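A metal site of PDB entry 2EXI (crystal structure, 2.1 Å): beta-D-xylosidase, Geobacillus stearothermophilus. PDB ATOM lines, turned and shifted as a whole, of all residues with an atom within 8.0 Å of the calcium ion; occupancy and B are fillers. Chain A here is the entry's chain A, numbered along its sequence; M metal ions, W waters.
NZ of Lys 395 is in salt-bridge range of OD1 of Asp 528.
The calcium ion is bound by O of Gly 362 (2.2 Å).
Water W2 is bound to the calcium ion (2.4 Å).
The calcium ion is bound by OD2 of Asp 528 (2.5 Å).
The calcium ion is bound by O of Asp 333, at 2.5 Å.
The backbone carbonyl oxygen (O) of Asp 528 binds the calcium ion, at 2.5 Å.
Water W1 binds the calcium ion (2.6 Å).
OD1 of Asp 333 binds the calcium ion (2.9 Å).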
ATOM      1  N   LYS A 331      -0.807  -3.687   8.584  1.00  0.00           N
ATOM      2  CA  LYS A 331       0.300  -3.267   7.743  1.00  0.00           C
ATOM      3  C   LYS A 331       0.889  -1.994   8.331  1.00  0.00           C
ATOM      4  O   LYS A 331       0.364  -0.904   8.101  1.00  0.00           O
ATOM      5  CB  LYS A 331      -0.150  -3.032   6.298  1.00  0.00           C
ATOM      6  CG  LYS A 331       0.960  -2.566   5.355  1.00  0.00           C
ATOM      7  CD  LYS A 331       0.580  -2.812   3.896  1.00  0.00           C
ATOM      8  CE  LYS A 331       1.609  -2.245   2.939  1.00  0.00           C
ATOM      9  NZ  LYS A 331       1.313  -2.632   1.526  1.00  0.00           N
ATOM     10  N   ASP A 332       1.959  -2.144   9.093  1.00  0.00           N
ATOM     11  CA  ASP A 332       2.623  -1.035   9.766  1.00  0.00           C
ATOM     12  C   ASP A 332       3.605  -0.389   8.803  1.00  0.00           C
ATOM     13  O   ASP A 332       4.654  -0.958   8.504  1.00  0.00           O
ATOM     14  CB  ASP A 332       3.305  -1.545  11.046  1.00  0.00           C
ATOM     15  CG  ASP A 332       4.034  -0.457  11.823  1.00  0.00           C
ATOM     16  OD1 ASP A 332       4.369   0.597  11.239  1.00  0.00           O
ATOM     17  OD2 ASP A 332       4.291  -0.671  13.027  1.00  0.00           O
ATOM     18  N   ASP A 333       3.260   0.797   8.312  1.00  0.00           N
ATOM     19  CA  ASP A 333       4.069   1.535   7.329  1.00  0.00           C
ATOM     20  C   ASP A 333       5.220   2.335   7.905  1.00  0.00           C
ATOM     21  O   ASP A 333       5.888   3.061   7.169  1.00  0.00           O
ATOM     22  CB  ASP A 333       3.180   2.484   6.516  1.00  0.00           C
ATOM     23  CG  ASP A 333       3.044   2.073   5.067  1.00  0.00           C
ATOM     24  OD1 ASP A 333       4.056   2.131   4.307  1.00  0.00           O
ATOM     25  OD2 ASP A 333       1.915   1.723   4.664  1.00  0.00           O
ATOM     26  N   PHE A 334       5.451   2.209   9.213  1.00  0.00           N
ATOM     27  CA  PHE A 334       6.485   2.982   9.907  1.00  0.00           C
ATOM     28  C   PHE A 334       6.294   4.479   9.711  1.00  0.00           C
ATOM     29  O   PHE A 334       7.192   5.172   9.237  1.00  0.00           O
ATOM     30  CB  PHE A 334       7.904   2.548   9.474  1.00  0.00           C
ATOM     31  CG  PHE A 334       8.201   1.091   9.721  1.00  0.00           C
ATOM     32  CD1 PHE A 334       8.043   0.532  10.986  1.00  0.00           C
ATOM     33  CD2 PHE A 334       8.649   0.271   8.684  1.00  0.00           C
ATOM     34  CE1 PHE A 334       8.318  -0.822  11.216  1.00  0.00           C
ATOM     35  CE2 PHE A 334       8.926  -1.081   8.901  1.00  0.00           C
ATOM     36  CZ  PHE A 334       8.750  -1.625  10.157  1.00  0.00           C
ATOM     37  N   ASP A 335       5.102   4.956  10.067  1.00  0.00           N
ATOM     38  CA  ASP A 335       4.700   6.355   9.884  1.00  0.00           C
ATOM     39  C   ASP A 335       4.992   7.221  11.104  1.00  0.00           C
ATOM     40  O   ASP A 335       5.077   8.446  10.987  1.00  0.00           O
ATOM     41  CB  ASP A 335       3.203   6.448   9.557  1.00  0.00           C
ATOM     42  CG  ASP A 335       2.838   5.850   8.198  1.00  0.00           C
ATOM     43  OD1 ASP A 335       3.641   5.975   7.237  1.00  0.00           O
ATOM     44  OD2 ASP A 335       1.732   5.271   8.099  1.00  0.00           O
ATOM     45  N   LEU A 357      13.968   5.785  12.398  1.00  0.00           N
ATOM     46  CA  LEU A 357      12.893   6.146  11.472  1.00  0.00           C
ATOM     47  C   LEU A 357      13.158   7.509  10.851  1.00  0.00           C
ATOM     48  O   LEU A 357      12.358   8.003  10.063  1.00  0.00           O
ATOM     49  CB  LEU A 357      11.557   6.171  12.207  1.00  0.00           C
ATOM     50  CG  LEU A 357      11.038   4.866  12.828  1.00  0.00           C
ATOM     51  CD1 LEU A 357       9.960   5.185  13.833  1.00  0.00           C
ATOM     52  CD2 LEU A 357      10.509   3.922  11.743  1.00  0.00           C
ATOM     53  N   ARG A 360      15.472   7.561   6.646  1.00  0.00           N
ATOM     54  CA  ARG A 360      14.659   7.495   5.441  1.00  0.00           C
ATOM     55  C   ARG A 360      13.194   7.560   5.812  1.00  0.00           C
ATOM     56  O   ARG A 360      12.672   6.614   6.396  1.00  0.00           O
ATOM     57  CB  ARG A 360      14.931   6.242   4.619  1.00  0.00           C
ATOM     58  CG  ARG A 360      14.339   6.344   3.232  1.00  0.00           C
ATOM     59  CD  ARG A 360      14.768   5.198   2.394  1.00  0.00           C
ATOM     60  NE  ARG A 360      14.065   5.186   1.119  1.00  0.00           N
ATOM     61  CZ  ARG A 360      14.326   4.323   0.146  1.00  0.00           C
ATOM     62  NH1 ARG A 360      15.285   3.415   0.299  1.00  0.00           N
ATOM     63  NH2 ARG A 360      13.629   4.385  -0.977  1.00  0.00           N
ATOM     64  N   PRO A 361      12.515   8.659   5.433  1.00  0.00           N
ATOM     65  CA  PRO A 361      11.136   8.867   5.868  1.00  0.00           C
ATOM     66  C   PRO A 361      10.247   7.672   5.544  1.00  0.00           C
ATOM     67  O   PRO A 361      10.358   7.086   4.468  1.00  0.00           O
ATOM     68  CB  PRO A 361      10.710  10.112   5.090  1.00  0.00           C
ATOM     69  CG  PRO A 361      11.988  10.828   4.794  1.00  0.00           C
ATOM     70  CD  PRO A 361      12.997   9.740   4.556  1.00  0.00           C
ATOM     71  N   GLY A 362       9.388   7.313   6.484  1.00  0.00           N
ATOM     72  CA  GLY A 362       8.484   6.171   6.298  1.00  0.00           C
ATOM     73  C   GLY A 362       9.179   4.824   6.177  1.00  0.00           C
ATOM     74  O   GLY A 362       8.582   3.867   5.691  1.00  0.00           O
ATOM     75  N   HIS A 363      10.425   4.744   6.622  1.00  0.00           N
ATOM     76  CA  HIS A 363      11.170   3.491   6.659  1.00  0.00           C
ATOM     77  C   HIS A 363      11.868   3.280   8.000  1.00  0.00           C
ATOM     78  O   HIS A 363      12.490   4.209   8.538  1.00  0.00           O
ATOM     79  CB  HIS A 363      12.259   3.481   5.590  1.00  0.00           C
ATOM     80  CG  HIS A 363      11.745   3.466   4.185  1.00  0.00           C
ATOM     81  ND1 HIS A 363      11.172   4.563   3.587  1.00  0.00           N
ATOM     82  CD2 HIS A 363      11.743   2.480   3.247  1.00  0.00           C
ATOM     83  CE1 HIS A 363      10.815   4.265   2.352  1.00  0.00           C
ATOM     84  NE2 HIS A 363      11.163   3.007   2.115  1.00  0.00           N
ATOM     85  N   LEU A 364      11.799   2.053   8.500  1.00  0.00           N
ATOM     86  CA  LEU A 364      12.732   1.633   9.533  1.00  0.00           C
ATOM     87  C   LEU A 364      14.051   1.261   8.870  1.00  0.00           C
ATOM     88  O   LEU A 364      14.131   0.313   8.065  1.00  0.00           O
ATOM     89  CB  LEU A 364      12.176   0.442  10.319  1.00  0.00           C
ATOM     90  CG  LEU A 364      13.124  -0.194  11.342  1.00  0.00           C
ATOM     91  CD1 LEU A 364      13.560   0.783  12.464  1.00  0.00           C
ATOM     92  CD2 LEU A 364      12.481  -1.449  11.909  1.00  0.00           C
ATOM     93  N   LYS A 395       9.107  -5.417   3.353  1.00  0.00           N
ATOM     94  CA  LYS A 395       9.542  -4.951   2.043  1.00  0.00           C
ATOM     95  C   LYS A 395      10.814  -4.174   2.312  1.00  0.00           C
ATOM     96  O   LYS A 395      10.805  -3.264   3.125  1.00  0.00           O
ATOM     97  CB  LYS A 395       8.462  -4.053   1.438  1.00  0.00           C
ATOM     98  CG  LYS A 395       8.858  -3.247   0.205  1.00  0.00           C
ATOM     99  CD  LYS A 395       7.775  -2.220  -0.094  1.00  0.00           C
ATOM    100  CE  LYS A 395       8.143  -1.326  -1.253  1.00  0.00           C
ATOM    101  NZ  LYS A 395       7.102  -0.283  -1.489  1.00  0.00           N
ATOM    102  N   TYR A 460      13.366  -2.909  -4.206  1.00  0.00           N
ATOM    103  CA  TYR A 460      12.798  -3.545  -3.031  1.00  0.00           C
ATOM    104  C   TYR A 460      12.570  -5.024  -3.241  1.00  0.00           C
ATOM    105  O   TYR A 460      12.065  -5.437  -4.278  1.00  0.00           O
ATOM    106  CB  TYR A 460      11.461  -2.899  -2.699  1.00  0.00           C
ATOM    107  CG  TYR A 460      11.531  -1.516  -2.099  1.00  0.00           C
ATOM    108  CD1 TYR A 460      11.941  -1.330  -0.776  1.00  0.00           C
ATOM    109  CD2 TYR A 460      11.141  -0.408  -2.840  1.00  0.00           C
ATOM    110  CE1 TYR A 460      11.985  -0.062  -0.215  1.00  0.00           C
ATOM    111  CE2 TYR A 460      11.182   0.866  -2.285  1.00  0.00           C
ATOM    112  CZ  TYR A 460      11.603   1.043  -0.976  1.00  0.00           C
ATOM    113  OH  TYR A 460      11.638   2.314  -0.438  1.00  0.00           O
ATOM    114  N   PHE A 527      13.475  -0.830   5.589  1.00  0.00           N
ATOM    115  CA  PHE A 527      12.226  -1.585   5.592  1.00  0.00           C
ATOM    116  C   PHE A 527      11.040  -0.611   5.454  1.00  0.00           C
ATOM    117  O   PHE A 527      10.859   0.273   6.285  1.00  0.00           O
ATOM    118  CB  PHE A 527      12.101  -2.424   6.877  1.00  0.00           C
ATOM    119  CG  PHE A 527      13.209  -3.464   7.047  1.00  0.00           C
ATOM    120  CD1 PHE A 527      13.001  -4.800   6.682  1.00  0.00           C
ATOM    121  CD2 PHE A 527      14.453  -3.106   7.570  1.00  0.00           C
ATOM    122  CE1 PHE A 527      14.003  -5.755   6.829  1.00  0.00           C
ATOM    123  CE2 PHE A 527      15.482  -4.061   7.709  1.00  0.00           C
ATOM    124  CZ  PHE A 527      15.242  -5.382   7.339  1.00  0.00           C
ATOM    125  N   ASP A 528      10.255  -0.774   4.392  1.00  0.00           N
ATOM    126  CA  ASP A 528       9.172   0.153   4.092  1.00  0.00           C
ATOM    127  C   ASP A 528       7.968  -0.087   5.008  1.00  0.00           C
ATOM    128  O   ASP A 528       7.371   0.856   5.536  1.00  0.00           O
ATOM    129  CB  ASP A 528       8.798   0.045   2.613  1.00  0.00           C
ATOM    130  CG  ASP A 528       7.852   1.130   2.148  1.00  0.00           C
ATOM    131  OD1 ASP A 528       7.163   0.858   1.147  1.00  0.00           O
ATOM    132  OD2 ASP A 528       7.786   2.235   2.754  1.00  0.00           O
ATOM    133  N   TYR A 529       7.635  -1.345   5.208  1.00  0.00           N
ATOM    134  CA  TYR A 529       6.580  -1.718   6.141  1.00  0.00           C
ATOM    135  C   TYR A 529       6.861  -3.050   6.815  1.00  0.00           C
ATOM    136  O   TYR A 529       7.750  -3.807   6.386  1.00  0.00           O
ATOM    137  CB  TYR A 529       5.211  -1.741   5.434  1.00  0.00           C
ATOM    138  CG  TYR A 529       5.049  -2.789   4.350  1.00  0.00           C
ATOM    139  CD1 TYR A 529       4.717  -4.107   4.664  1.00  0.00           C
ATOM    140  CD2 TYR A 529       5.197  -2.450   3.003  1.00  0.00           C
ATOM    141  CE1 TYR A 529       4.572  -5.073   3.678  1.00  0.00           C
ATOM    142  CE2 TYR A 529       5.031  -3.412   1.998  1.00  0.00           C
ATOM    143  CZ  TYR A 529       4.725  -4.708   2.343  1.00  0.00           C
ATOM    144  OH  TYR A 529       4.556  -5.655   1.355  1.00  0.00           O
ATOM    145  N   PHE A 530       6.110  -3.330   7.877  1.00  0.00           N
ATOM    146  CA  PHE A 530       6.076  -4.648   8.481  1.00  0.00           C
ATOM    147  C   PHE A 530       4.624  -5.021   8.738  1.00  0.00           C
ATOM    148  O   PHE A 530       3.907  -4.334   9.455  1.00  0.00           O
ATOM    149  CB  PHE A 530       6.870  -4.738   9.780  1.00  0.00           C
ATOM    150  CG  PHE A 530       6.925  -6.124  10.354  1.00  0.00           C
ATOM    151  CD1 PHE A 530       7.934  -6.999   9.967  1.00  0.00           C
ATOM    152  CD2 PHE A 530       5.972  -6.567  11.253  1.00  0.00           C
ATOM    153  CE1 PHE A 530       7.996  -8.287  10.478  1.00  0.00           C
ATOM    154  CE2 PHE A 530       6.028  -7.867  11.768  1.00  0.00           C
ATOM    155  CZ  PHE A 530       7.040  -8.722  11.371  1.00  0.00           C
HETATM  156 CA    CA M   1       6.686   3.181   4.787  1.00  0.00          CA
HETATM  157  O   HOH W   1       5.199   5.265   5.222  1.00  0.00           O
HETATM  158  O   HOH W   2       6.812   4.828   3.072  1.00  0.00           O
